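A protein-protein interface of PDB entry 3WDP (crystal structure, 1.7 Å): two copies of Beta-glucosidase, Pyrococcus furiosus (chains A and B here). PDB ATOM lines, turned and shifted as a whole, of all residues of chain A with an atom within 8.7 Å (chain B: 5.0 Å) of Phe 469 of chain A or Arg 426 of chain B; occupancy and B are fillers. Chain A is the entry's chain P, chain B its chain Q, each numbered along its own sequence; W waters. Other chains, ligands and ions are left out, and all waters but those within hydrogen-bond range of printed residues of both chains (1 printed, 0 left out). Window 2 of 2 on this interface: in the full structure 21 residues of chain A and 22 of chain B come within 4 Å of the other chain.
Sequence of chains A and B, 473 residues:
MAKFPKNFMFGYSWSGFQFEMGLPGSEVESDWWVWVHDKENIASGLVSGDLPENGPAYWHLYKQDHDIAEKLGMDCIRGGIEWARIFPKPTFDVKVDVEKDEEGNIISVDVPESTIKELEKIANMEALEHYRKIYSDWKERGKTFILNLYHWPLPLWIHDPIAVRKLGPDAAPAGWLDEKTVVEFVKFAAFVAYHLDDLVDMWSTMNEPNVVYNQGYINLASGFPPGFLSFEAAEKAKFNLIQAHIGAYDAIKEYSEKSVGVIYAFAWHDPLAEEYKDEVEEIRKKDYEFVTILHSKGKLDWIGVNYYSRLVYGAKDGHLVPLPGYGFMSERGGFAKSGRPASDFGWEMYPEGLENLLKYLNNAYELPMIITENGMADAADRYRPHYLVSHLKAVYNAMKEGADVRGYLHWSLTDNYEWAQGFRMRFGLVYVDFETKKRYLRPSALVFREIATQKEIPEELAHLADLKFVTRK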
ATOM      1  N   PHE A 335     -12.029 -17.763  16.887  1.00  0.00           N
ATOM      2  CA  PHE A 335     -11.876 -18.491  15.646  1.00  0.00           C
ATOM      3  C   PHE A 335     -12.710 -17.898  14.530  1.00  0.00           C
ATOM      4  O   PHE A 335     -13.844 -17.472  14.739  1.00  0.00           O
ATOM      5  CB  PHE A 335     -12.256 -19.971  15.874  1.00  0.00           C
ATOM      6  CG  PHE A 335     -11.305 -20.660  16.786  1.00  0.00           C
ATOM      7  CD1 PHE A 335     -10.153 -21.241  16.282  1.00  0.00           C
ATOM      8  CD2 PHE A 335     -11.498 -20.639  18.154  1.00  0.00           C
ATOM      9  CE1 PHE A 335      -9.232 -21.848  17.130  1.00  0.00           C
ATOM     10  CE2 PHE A 335     -10.579 -21.217  19.011  1.00  0.00           C
ATOM     11  CZ  PHE A 335      -9.439 -21.820  18.504  1.00  0.00           C
ATOM     12  N   GLY A 339     -12.473 -21.994  10.881  1.00  0.00           N
ATOM     13  CA  GLY A 339     -11.870 -22.775  11.955  1.00  0.00           C
ATOM     14  C   GLY A 339     -10.474 -22.279  12.289  1.00  0.00           C
ATOM     15  O   GLY A 339      -9.883 -22.678  13.275  1.00  0.00           O
ATOM     16  N   ARG A 340      -9.924 -21.375  11.469  1.00  0.00           N
ATOM     17  CA  ARG A 340      -8.609 -20.825  11.768  1.00  0.00           C
ATOM     18  C   ARG A 340      -8.642 -19.919  13.011  1.00  0.00           C
ATOM     19  O   ARG A 340      -9.617 -19.214  13.238  1.00  0.00           O
ATOM     20  CB  ARG A 340      -8.089 -20.004  10.589  1.00  0.00           C
ATOM     21  CG  ARG A 340      -7.656 -20.818   9.391  1.00  0.00           C
ATOM     22  CD  ARG A 340      -6.291 -21.425   9.611  1.00  0.00           C
ATOM     23  NE  ARG A 340      -5.957 -22.383   8.558  1.00  0.00           N
ATOM     24  CZ  ARG A 340      -5.432 -22.073   7.373  1.00  0.00           C
ATOM     25  NH1 ARG A 340      -5.144 -20.810   7.061  1.00  0.00           N
ATOM     26  NH2 ARG A 340      -5.167 -23.040   6.501  1.00  0.00           N
ATOM     27  N   PRO A 341      -7.568 -19.918  13.792  1.00  0.00           N
ATOM     28  CA  PRO A 341      -7.521 -19.029  14.934  1.00  0.00           C
ATOM     29  C   PRO A 341      -7.496 -17.558  14.472  1.00  0.00           C
ATOM     30  O   PRO A 341      -6.959 -17.265  13.415  1.00  0.00           O
ATOM     31  CB  PRO A 341      -6.223 -19.420  15.634  1.00  0.00           C
ATOM     32  CG  PRO A 341      -5.377 -20.039  14.581  1.00  0.00           C
ATOM     33  CD  PRO A 341      -6.335 -20.723  13.654  1.00  0.00           C
ATOM     34  N   ARG A 382       0.771 -17.546  22.034  1.00  0.00           N
ATOM     35  CA  ARG A 382       0.166 -18.847  21.823  1.00  0.00           C
ATOM     36  C   ARG A 382       0.177 -19.248  20.361  1.00  0.00           C
ATOM     37  O   ARG A 382       0.296 -20.425  20.041  1.00  0.00           O
ATOM     38  CB  ARG A 382      -1.260 -18.894  22.335  1.00  0.00           C
ATOM     39  CG  ARG A 382      -1.358 -18.757  23.843  1.00  0.00           C
ATOM     40  CD  ARG A 382      -2.797 -18.900  24.240  1.00  0.00           C
ATOM     41  NE  ARG A 382      -3.586 -17.825  23.670  1.00  0.00           N
ATOM     42  CZ  ARG A 382      -4.913 -17.818  23.630  1.00  0.00           C
ATOM     43  NH1 ARG A 382      -5.614 -18.832  24.148  1.00  0.00           N
ATOM     44  NH2 ARG A 382      -5.544 -16.776  23.081  1.00  0.00           N
ATOM     45  N   TYR A 383       0.067 -18.264  19.478  1.00  0.00           N
ATOM     46  CA  TYR A 383      -0.144 -18.529  18.082  1.00  0.00           C
ATOM     47  C   TYR A 383       0.946 -18.001  17.156  1.00  0.00           C
ATOM     48  O   TYR A 383       1.095 -18.466  16.028  1.00  0.00           O
ATOM     49  CB  TYR A 383      -1.441 -17.913  17.702  1.00  0.00           C
ATOM     50  CG  TYR A 383      -2.632 -18.656  18.252  1.00  0.00           C
ATOM     51  CD1 TYR A 383      -2.975 -19.905  17.746  1.00  0.00           C
ATOM     52  CD2 TYR A 383      -3.416 -18.110  19.253  1.00  0.00           C
ATOM     53  CE1 TYR A 383      -4.074 -20.588  18.220  1.00  0.00           C
ATOM     54  CE2 TYR A 383      -4.536 -18.791  19.728  1.00  0.00           C
ATOM     55  CZ  TYR A 383      -4.845 -20.026  19.201  1.00  0.00           C
ATOM     56  OH  TYR A 383      -5.931 -20.734  19.658  1.00  0.00           O
ATOM     57  N   HIS A 386       3.296 -20.281  14.964  1.00  0.00           N
ATOM     58  CA  HIS A 386       2.640 -20.845  13.803  1.00  0.00           C
ATOM     59  C   HIS A 386       2.443 -19.740  12.734  1.00  0.00           C
ATOM     60  O   HIS A 386       2.650 -19.948  11.544  1.00  0.00           O
ATOM     61  CB  HIS A 386       1.302 -21.515  14.169  1.00  0.00           C
ATOM     62  CG  HIS A 386       1.435 -22.921  14.670  1.00  0.00           C
ATOM     63  ND1 HIS A 386       1.450 -23.229  16.013  1.00  0.00           N
ATOM     64  CD2 HIS A 386       1.484 -24.103  14.016  1.00  0.00           C
ATOM     65  CE1 HIS A 386       1.564 -24.541  16.166  1.00  0.00           C
ATOM     66  NE2 HIS A 386       1.566 -25.097  14.971  1.00  0.00           N
ATOM     67  N   HIS A 463       6.915 -28.191  10.786  1.00  0.00           N
ATOM     68  CA  HIS A 463       5.554 -28.458  11.222  1.00  0.00           C
ATOM     69  C   HIS A 463       4.861 -27.196  11.787  1.00  0.00           C
ATOM     70  O   HIS A 463       3.635 -27.141  11.906  1.00  0.00           O
ATOM     71  CB  HIS A 463       5.517 -29.626  12.217  1.00  0.00           C
ATOM     72  CG  HIS A 463       4.131 -30.057  12.561  1.00  0.00           C
ATOM     73  ND1 HIS A 463       3.581 -29.878  13.808  1.00  0.00           N
ATOM     74  CD2 HIS A 463       3.167 -30.625  11.803  1.00  0.00           C
ATOM     75  CE1 HIS A 463       2.346 -30.342  13.815  1.00  0.00           C
ATOM     76  NE2 HIS A 463       2.062 -30.775  12.603  1.00  0.00           N
ATOM     77  N   ALA A 465       4.613 -24.624  10.083  1.00  0.00           N
ATOM     78  CA  ALA A 465       3.853 -24.093   8.932  1.00  0.00           C
ATOM     79  C   ALA A 465       2.491 -24.755   8.788  1.00  0.00           C
ATOM     80  O   ALA A 465       1.632 -24.257   8.082  1.00  0.00           O
ATOM     81  CB  ALA A 465       4.641 -24.239   7.648  1.00  0.00           C
ATOM     82  N   ASP A 466       2.294 -25.891   9.457  1.00  0.00           N
ATOM     83  CA  ASP A 466       1.058 -26.655   9.364  1.00  0.00           C
ATOM     84  C   ASP A 466       0.097 -26.184  10.431  1.00  0.00           C
ATOM     85  O   ASP A 466       0.399 -26.271  11.624  1.00  0.00           O
ATOM     86  CB  ASP A 466       1.394 -28.146   9.571  1.00  0.00           C
ATOM     87  CG  ASP A 466       0.212 -29.067   9.369  1.00  0.00           C
ATOM     88  OD1 ASP A 466      -0.951 -28.642   9.451  1.00  0.00           O
ATOM     89  OD2 ASP A 466       0.461 -30.269   9.126  1.00  0.00           O
ATOM     90  N   LEU A 467      -1.075 -25.719  10.020  1.00  0.00           N
ATOM     91  CA  LEU A 467      -2.023 -25.121  10.970  1.00  0.00           C
ATOM     92  C   LEU A 467      -3.095 -26.089  11.538  1.00  0.00           C
ATOM     93  O   LEU A 467      -4.007 -25.667  12.235  1.00  0.00           O
ATOM     94  CB  LEU A 467      -2.636 -23.861  10.357  1.00  0.00           C
ATOM     95  CG  LEU A 467      -1.602 -22.778   9.949  1.00  0.00           C
ATOM     96  CD1 LEU A 467      -2.323 -21.485   9.593  1.00  0.00           C
ATOM     97  CD2 LEU A 467      -0.581 -22.506  11.038  1.00  0.00           C
ATOM     98  N   LYS A 468      -2.930 -27.390  11.305  1.00  0.00           N
ATOM     99  CA  LYS A 468      -3.923 -28.387  11.730  1.00  0.00           C
ATOM    100  C   LYS A 468      -4.218 -28.323  13.220  1.00  0.00           C
ATOM    101  O   LYS A 468      -5.386 -28.299  13.627  1.00  0.00           O
ATOM    102  CB  LYS A 468      -3.436 -29.803  11.376  1.00  0.00           C
ATOM    103  CG  LYS A 468      -4.390 -30.924  11.803  1.00  0.00           C
ATOM    104  CD  LYS A 468      -3.795 -32.322  11.625  1.00  0.00           C
ATOM    105  CE  LYS A 468      -3.424 -32.616  10.181  1.00  0.00           C
ATOM    106  NZ  LYS A 468      -3.103 -34.058   9.937  1.00  0.00           N
ATOM    107  N   PHE A 469      -3.180 -28.272  14.052  1.00  0.00           N
ATOM    108  CA  PHE A 469      -3.410 -28.349  15.501  1.00  0.00           C
ATOM    109  C   PHE A 469      -3.824 -27.037  16.150  1.00  0.00           C
ATOM    110  O   PHE A 469      -4.142 -27.008  17.346  1.00  0.00           O
ATOM    111  CB  PHE A 469      -2.207 -28.986  16.224  1.00  0.00           C
ATOM    112  CG  PHE A 469      -2.037 -30.462  15.912  1.00  0.00           C
ATOM    113  CD1 PHE A 469      -2.752 -31.403  16.602  1.00  0.00           C
ATOM    114  CD2 PHE A 469      -1.201 -30.881  14.887  1.00  0.00           C
ATOM    115  CE1 PHE A 469      -2.617 -32.753  16.322  1.00  0.00           C
ATOM    116  CE2 PHE A 469      -1.049 -32.230  14.597  1.00  0.00           C
ATOM    117  CZ  PHE A 469      -1.763 -33.168  15.321  1.00  0.00           C
ATOM    118  N   VAL A 470      -3.890 -25.951  15.362  1.00  0.00           N
ATOM    119  CA  VAL A 470      -4.479 -24.704  15.846  1.00  0.00           C
ATOM    120  C   VAL A 470      -5.853 -24.407  15.236  1.00  0.00           C
ATOM    121  O   VAL A 470      -6.535 -23.472  15.648  1.00  0.00           O
ATOM    122  CB  VAL A 470      -3.531 -23.512  15.635  1.00  0.00           C
ATOM    123  CG1 VAL A 470      -2.214 -23.739  16.393  1.00  0.00           C
ATOM    124  CG2 VAL A 470      -3.303 -23.226  14.154  1.00  0.00           C
ATOM    125  N   THR A 471      -6.259 -25.216  14.271  1.00  0.00           N
ATOM    126  CA  THR A 471      -7.487 -24.995  13.522  1.00  0.00           C
ATOM    127  C   THR A 471      -8.625 -25.876  14.054  1.00  0.00           C
ATOM    128  O   THR A 471      -8.486 -27.098  14.120  1.00  0.00           O
ATOM    129  CB  THR A 471      -7.237 -25.274  12.041  1.00  0.00           C
ATOM    130  OG1 THR A 471      -6.235 -24.374  11.568  1.00  0.00           O
ATOM    131  CG2 THR A 471      -8.486 -25.092  11.219  1.00  0.00           C
ATOM    132  N   ARG A 472      -9.741 -25.246  14.420  1.00  0.00           N
ATOM    133  CA  ARG A 472     -10.873 -25.966  15.008  1.00  0.00           C
ATOM    134  C   ARG A 472     -11.614 -26.833  14.000  1.00  0.00           C
ATOM    135  O   ARG A 472     -11.902 -26.400  12.881  1.00  0.00           O
ATOM    136  CB  ARG A 472     -11.861 -25.019  15.694  1.00  0.00           C
ATOM    137  CG  ARG A 472     -11.508 -24.708  17.146  1.00  0.00           C
ATOM    138  CD  ARG A 472     -12.693 -24.872  18.098  1.00  0.00           C
ATOM    139  NE  ARG A 472     -13.341 -23.607  18.448  1.00  0.00           N
ATOM    140  CZ  ARG A 472     -14.255 -22.971  17.714  1.00  0.00           C
ATOM    141  NH1 ARG A 472     -14.662 -23.447  16.539  1.00  0.00           N
ATOM    142  NH2 ARG A 472     -14.765 -21.828  18.158  1.00  0.00           N
ATOM    143  N   LYS A 473     -11.887 -28.066  14.437  1.00  0.00           N
ATOM    144  CA  LYS A 473     -12.719 -29.065  13.748  1.00  0.00           C
ATOM    145  C   LYS A 473     -12.416 -29.249  12.265  1.00  0.00           C
ATOM    146  O   LYS A 473     -11.505 -30.003  11.916  1.00  0.00           O
ATOM    147  CB  LYS A 473     -14.211 -28.774  13.981  1.00  0.00           C
ATOM    148  CG  LYS A 473     -14.538 -28.317  15.400  1.00  0.00           C
ATOM    149  CD  LYS A 473     -14.042 -29.291  16.468  1.00  0.00           C
ATOM    150  CE  LYS A 473     -13.709 -28.586  17.777  1.00  0.00           C
ATOM    151  NZ  LYS A 473     -14.905 -27.969  18.411  1.00  0.00           N
ATOM    152  OXT LYS A 473     -13.065 -28.679  11.386  1.00  0.00           O
ATOM    153  N   MET B 376       2.465 -31.185  30.025  1.00  0.00           N
ATOM    154  CA  MET B 376       1.103 -30.901  29.690  1.00  0.00           C
ATOM    155  C   MET B 376       0.724 -31.388  28.302  1.00  0.00           C
ATOM    156  O   MET B 376       1.531 -31.446  27.400  1.00  0.00           O
ATOM    157  CB  MET B 376       0.768 -29.413  29.892  1.00  0.00           C
ATOM    158  CG  MET B 376       1.236 -28.482  28.803  1.00  0.00           C
ATOM    159  SD  MET B 376       0.534 -26.814  28.996  1.00  0.00           S
ATOM    160  CE  MET B 376      -1.224 -27.024  28.936  1.00  0.00           C
ATOM    161  N   ALA B 377      -0.534 -31.793  28.197  1.00  0.00           N
ATOM    162  CA  ALA B 377      -1.166 -32.154  26.921  1.00  0.00           C
ATOM    163  C   ALA B 377      -1.482 -30.852  26.218  1.00  0.00           C
ATOM    164  O   ALA B 377      -2.317 -30.050  26.685  1.00  0.00           O
ATOM    165  CB  ALA B 377      -2.407 -32.980  27.158  1.00  0.00           C
ATOM    166  N   ASP B 378      -0.759 -30.617  25.132  1.00  0.00           N
ATOM    167  CA  ASP B 378      -0.805 -29.327  24.429  1.00  0.00           C
ATOM    168  C   ASP B 378      -0.361 -29.570  22.988  1.00  0.00           C
ATOM    169  O   ASP B 378       0.814 -29.472  22.648  1.00  0.00           O
ATOM    170  CB  ASP B 378       0.133 -28.359  25.179  1.00  0.00           C
ATOM    171  CG  ASP B 378      -0.106 -26.899  24.840  1.00  0.00           C
ATOM    172  OD1 ASP B 378      -1.252 -26.520  24.528  1.00  0.00           O
ATOM    173  OD2 ASP B 378       0.862 -26.133  24.899  1.00  0.00           O
ATOM    174  N   ALA B 379      -1.308 -29.930  22.128  1.00  0.00           N
ATOM    175  CA  ALA B 379      -0.954 -30.417  20.813  1.00  0.00           C
ATOM    176  C   ALA B 379      -0.373 -29.338  19.873  1.00  0.00           C
ATOM    177  O   ALA B 379       0.321 -29.661  18.929  1.00  0.00           O
ATOM    178  CB  ALA B 379      -2.157 -31.145  20.168  1.00  0.00           C
ATOM    179  N   ALA B 380      -0.599 -28.072  20.173  1.00  0.00           N
ATOM    180  CA  ALA B 380      -0.060 -26.988  19.331  1.00  0.00           C
ATOM    181  C   ALA B 380       1.016 -26.155  20.039  1.00  0.00           C
ATOM    182  O   ALA B 380       1.458 -25.153  19.508  1.00  0.00           O
ATOM    183  CB  ALA B 380      -1.196 -26.079  18.907  1.00  0.00           C
ATOM    184  N   ARG B 384       2.541 -24.778  26.609  1.00  0.00           N
ATOM    185  CA  ARG B 384       3.731 -25.478  27.147  1.00  0.00           C
ATOM    186  C   ARG B 384       4.892 -24.585  27.542  1.00  0.00           C
ATOM    187  O   ARG B 384       5.565 -24.838  28.561  1.00  0.00           O
ATOM    188  CB  ARG B 384       4.259 -26.502  26.182  1.00  0.00           C
ATOM    189  CG  ARG B 384       5.198 -27.490  26.863  1.00  0.00           C
ATOM    190  CD  ARG B 384       5.522 -28.671  25.992  1.00  0.00           C
ATOM    191  NE  ARG B 384       4.434 -29.624  25.895  1.00  0.00           N
ATOM    192  CZ  ARG B 384       3.602 -29.767  24.869  1.00  0.00           C
ATOM    193  NH1 ARG B 384       3.664 -28.983  23.796  1.00  0.00           N
ATOM    194  NH2 ARG B 384       2.679 -30.692  24.928  1.00  0.00           N
ATOM    195  N   ASP B 415       5.778 -36.577  21.862  1.00  0.00           N
ATOM    196  CA  ASP B 415       4.440 -37.206  21.937  1.00  0.00           C
ATOM    197  C   ASP B 415       4.499 -38.754  21.986  1.00  0.00           C
ATOM    198  O   ASP B 415       5.412 -39.385  21.442  1.00  0.00           O
ATOM    199  CB  ASP B 415       3.561 -36.797  20.758  1.00  0.00           C
ATOM    200  CG  ASP B 415       3.375 -35.319  20.661  1.00  0.00           C
ATOM    201  OD1 ASP B 415       3.508 -34.657  21.715  1.00  0.00           O
ATOM    202  OD2 ASP B 415       3.101 -34.867  19.529  1.00  0.00           O
ATOM    203  N   PHE B 423      -3.484 -41.293  21.423  1.00  0.00           N
ATOM    204  CA  PHE B 423      -2.524 -40.337  20.920  1.00  0.00           C
ATOM    205  C   PHE B 423      -3.038 -38.904  21.033  1.00  0.00           C
ATOM    206  O   PHE B 423      -2.263 -37.967  20.835  1.00  0.00           O
ATOM    207  CB  PHE B 423      -2.134 -40.658  19.474  1.00  0.00           C
ATOM    208  CG  PHE B 423      -1.361 -41.940  19.335  1.00  0.00           C
ATOM    209  CD1 PHE B 423      -0.110 -42.071  19.903  1.00  0.00           C
ATOM    210  CD2 PHE B 423      -1.902 -43.020  18.672  1.00  0.00           C
ATOM    211  CE1 PHE B 423       0.586 -43.264  19.816  1.00  0.00           C
ATOM    212  CE2 PHE B 423      -1.208 -44.194  18.567  1.00  0.00           C
ATOM    213  CZ  PHE B 423       0.019 -44.336  19.157  1.00  0.00           C
ATOM    214  N   ARG B 424      -4.304 -38.715  21.404  1.00  0.00           N
ATOM    215  CA  ARG B 424      -4.867 -37.366  21.359  1.00  0.00           C
ATOM    216  C   ARG B 424      -4.293 -36.426  22.413  1.00  0.00           C
ATOM    217  O   ARG B 424      -4.377 -35.214  22.254  1.00  0.00           O
ATOM    218  CB  ARG B 424      -6.387 -37.385  21.434  1.00  0.00           C
ATOM    219  CG  ARG B 424      -6.981 -37.671  22.794  1.00  0.00           C
ATOM    220  CD  ARG B 424      -8.499 -37.491  22.776  1.00  0.00           C
ATOM    221  NE  ARG B 424      -9.127 -38.530  21.964  1.00  0.00           N
ATOM    222  CZ  ARG B 424      -9.572 -39.712  22.408  1.00  0.00           C
ATOM    223  NH1 ARG B 424      -9.500 -40.060  23.698  1.00  0.00           N
ATOM    224  NH2 ARG B 424     -10.098 -40.567  21.535  1.00  0.00           N
ATOM    225  N   MET B 425      -3.734 -36.989  23.485  1.00  0.00           N
ATOM    226  CA  MET B 425      -2.993 -36.229  24.490  1.00  0.00           C
ATOM    227  C   MET B 425      -1.492 -36.204  24.110  1.00  0.00           C
ATOM    228  O   MET B 425      -0.807 -37.195  24.169  1.00  0.00           O
ATOM    229  CB  MET B 425      -3.239 -36.819  25.881  1.00  0.00           C
ATOM    230  CG  MET B 425      -4.683 -36.872  26.325  1.00  0.00           C
ATOM    231  SD  MET B 425      -5.506 -35.270  26.178  1.00  0.00           S
ATOM    232  CE  MET B 425      -7.178 -35.750  26.611  1.00  0.00           C
ATOM    233  N   ARG B 426      -0.999 -35.041  23.697  1.00  0.00           N
ATOM    234  CA  ARG B 426       0.359 -34.903  23.143  1.00  0.00           C
ATOM    235  C   ARG B 426       1.197 -34.089  24.096  1.00  0.00           C
ATOM    236  O   ARG B 426       1.044 -32.849  24.214  1.00  0.00           O
ATOM    237  CB  ARG B 426       0.297 -34.205  21.769  1.00  0.00           C
ATOM    238  CG  ARG B 426      -0.191 -35.113  20.644  1.00  0.00           C
ATOM    239  CD  ARG B 426      -0.359 -34.414  19.297  1.00  0.00           C
ATOM    240  NE  ARG B 426      -0.779 -35.353  18.251  1.00  0.00           N
ATOM    241  CZ  ARG B 426       0.034 -36.116  17.526  1.00  0.00           C
ATOM    242  NH1 ARG B 426       1.347 -36.136  17.735  1.00  0.00           N
ATOM    243  NH2 ARG B 426      -0.479 -36.898  16.596  1.00  0.00           N
ATOM    244  N   PHE B 427       2.101 -34.770  24.800  1.00  0.00           N
ATOM    245  CA  PHE B 427       2.860 -34.176  25.890  1.00  0.00           C
ATOM    246  C   PHE B 427       4.291 -33.773  25.500  1.00  0.00           C
ATOM    247  O   PHE B 427       5.144 -33.415  26.390  1.00  0.00           O
ATOM    248  CB  PHE B 427       2.956 -35.190  27.063  1.00  0.00           C
ATOM    249  CG  PHE B 427       1.781 -35.212  27.987  1.00  0.00           C
ATOM    250  CD1 PHE B 427       0.705 -36.016  27.740  1.00  0.00           C
ATOM    251  CD2 PHE B 427       1.796 -34.477  29.166  1.00  0.00           C
ATOM    252  CE1 PHE B 427      -0.383 -36.047  28.619  1.00  0.00           C
ATOM    253  CE2 PHE B 427       0.751 -34.526  30.038  1.00  0.00           C
ATOM    254  CZ  PHE B 427      -0.322 -35.345  29.813  1.00  0.00           C
ATOM    255  N   GLY B 428       4.645 -33.945  24.224  1.00  0.00           N
ATOM    256  CA  GLY B 428       6.038 -33.730  23.796  1.00  0.00           C
ATOM    257  C   GLY B 428       6.538 -32.291  23.724  1.00  0.00           C
ATOM    258  O   GLY B 428       5.826 -31.412  23.285  1.00  0.00           O
ATOM    259  N   TYR B 431       6.930 -32.837  18.537  1.00  0.00           N
ATOM    260  CA  TYR B 431       5.759 -33.411  17.907  1.00  0.00           C
ATOM    261  C   TYR B 431       6.206 -34.627  17.150  1.00  0.00           C
ATOM    262  O   TYR B 431       7.269 -34.612  16.508  1.00  0.00           O
ATOM    263  CB  TYR B 431       5.111 -32.386  16.977  1.00  0.00           C
ATOM    264  CG  TYR B 431       4.215 -32.967  15.875  1.00  0.00           C
ATOM    265  CD1 TYR B 431       2.953 -33.411  16.154  1.00  0.00           C
ATOM    266  CD2 TYR B 431       4.660 -33.027  14.558  1.00  0.00           C
ATOM    267  CE1 TYR B 431       2.131 -33.955  15.170  1.00  0.00           C
ATOM    268  CE2 TYR B 431       3.858 -33.563  13.549  1.00  0.00           C
ATOM    269  CZ  TYR B 431       2.579 -34.006  13.867  1.00  0.00           C
ATOM    270  OH  TYR B 431       1.721 -34.524  12.914  1.00  0.00           O
ATOM    271  N   VAL B 432       5.407 -35.689  17.219  1.00  0.00           N
ATOM    272  CA  VAL B 432       5.630 -36.879  16.382  1.00  0.00           C
ATOM    273  C   VAL B 432       4.449 -37.093  15.464  1.00  0.00           C
ATOM    274  O   VAL B 432       3.293 -37.144  15.933  1.00  0.00           O
ATOM    275  CB  VAL B 432       5.871 -38.154  17.257  1.00  0.00           C
ATOM    276  CG1 VAL B 432       5.927 -39.394  16.388  1.00  0.00           C
ATOM    277  CG2 VAL B 432       7.142 -37.923  18.099  1.00  0.00           C
ATOM    278  N   PHE B 434       2.690 -39.732  13.802  1.00  0.00           N
ATOM    279  CA  PHE B 434       2.655 -41.175  14.055  1.00  0.00           C
ATOM    280  C   PHE B 434       2.512 -42.005  12.778  1.00  0.00           C
ATOM    281  O   PHE B 434       2.771 -43.205  12.779  1.00  0.00           O
ATOM    282  CB  PHE B 434       1.596 -41.525  15.097  1.00  0.00           C
ATOM    283  CG  PHE B 434       1.929 -41.004  16.490  1.00  0.00           C
ATOM    284  CD1 PHE B 434       3.012 -41.511  17.186  1.00  0.00           C
ATOM    285  CD2 PHE B 434       1.145 -40.013  17.093  1.00  0.00           C
ATOM    286  CE1 PHE B 434       3.322 -41.045  18.479  1.00  0.00           C
ATOM    287  CE2 PHE B 434       1.445 -39.526  18.376  1.00  0.00           C
ATOM    288  CZ  PHE B 434       2.545 -40.049  19.050  1.00  0.00           C
ATOM    289  N   ARG B 442       8.891 -28.379  18.870  1.00  0.00           N
ATOM    290  CA  ARG B 442       7.981 -27.306  19.252  1.00  0.00           C
ATOM    291  C   ARG B 442       8.799 -26.182  19.853  1.00  0.00           C
ATOM    292  O   ARG B 442       9.917 -26.402  20.295  1.00  0.00           O
ATOM    293  CB  ARG B 442       6.947 -27.818  20.236  1.00  0.00           C
ATOM    294  CG  ARG B 442       6.021 -28.860  19.655  1.00  0.00           C
ATOM    295  CD  ARG B 442       4.943 -29.271  20.623  1.00  0.00           C
ATOM    296  NE  ARG B 442       3.940 -30.076  19.949  1.00  0.00           N
ATOM    297  CZ  ARG B 442       3.586 -31.330  20.227  1.00  0.00           C
ATOM    298  NH1 ARG B 442       4.107 -32.022  21.288  1.00  0.00           N
ATOM    299  NH2 ARG B 442       2.631 -31.888  19.451  1.00  0.00           N
HETATM  300  O   HOH W   1       3.634 -23.183  18.735  1.00  0.00           O
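Water W1 lies within hydrogen-bond range of O of Ala 380 of chain B (3.0 Å) and ND1 of His 386 of chain A (3.5 Å).
Among the printed residues, merely in contact across the chains: His 386 of chain A with Ala 380 of chain B, His 463 of chain A with Tyr 431 of chain B, Phe 469 of chain A with Ala 379 of chain B, Phe 469 of chain A with Ala 380 of chain B, Phe 469 of chain A with Arg 426 of chain B, Phe 469 of chain A with Tyr 431 of chain B and Val 470 of chain A with Ala 380 of chain B.
No position is printed for both chains.
Of the 17 printed residues of chain B, 4 touch a printed residue of chain A. Printed residues of chain B that touch a printed residue of chain A: Ala 379, Ala 380, Arg 426 and Tyr 431. Hydrophobic or aromatic side chains of chain B that line the printed part of chain A: Ala 379, Ala 380 and Tyr 431. Of the 17 printed residues of chain A, 4 touch a printed residue of chain B. Hydrophobic or aromatic side chains of chain A within 4 Å of the printed part of chain B: His 386, His 463, Phe 469 and Val 470.
Printed residues of chain B within 4 Å of His 463 of chain A: Tyr 431 (3.4 Å). Of chain B, only Ala 379 (3.6 Å), Ala 380 (3.5 Å), Arg 426 (3.7 Å) and Tyr 431 (3.7 Å) come within 4 Å of Phe 469 of chain A. Ala 379 of chain B touches just one residue of chain A: Phe 469. Arg 426 of chain B touches just one residue of chain A: Phe 469 (3.7 Å). Of the printed residues of chain A, Tyr 431 of chain B touches His 463 (3.4 Å) and Phe 469 (3.7 Å). The nearest residue of chain A that does not touch Arg 426 of chain B is His 463 of chain A (7.1 Å). The nearest printed residue of chain B that does not touch His 463 of chain A is Ala 379 of chain B (5.5 Å).
The side-chain carboxylate of Asp 415 of chain B lies within salt-bridge range of the guanidinium group of Arg 426 of chain B (2.8 Å). The backbone carbonyl oxygen (O) of Ala 379 of chain B is in hydrogen-bond range of the guanidinium group (NH2) of Arg 442 of chain B (3.3 Å). The guanidinium group of Arg 426 of chain B is in hydrogen-bond range of the backbone carbonyl oxygen of Val 432 of chain B, 2.8 Å away. The guanidinium group (NH2) of Arg 384 of chain B sits at hydrogen-bond distance from the backbone carbonyl oxygen (O) of Arg 426 of chain B, at 2.8 Å. The backbone carbonyl oxygen of Arg 426 of chain B lies within hydrogen-bond range of the backbone NH of Asp 378 of chain B (3.0 Å).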
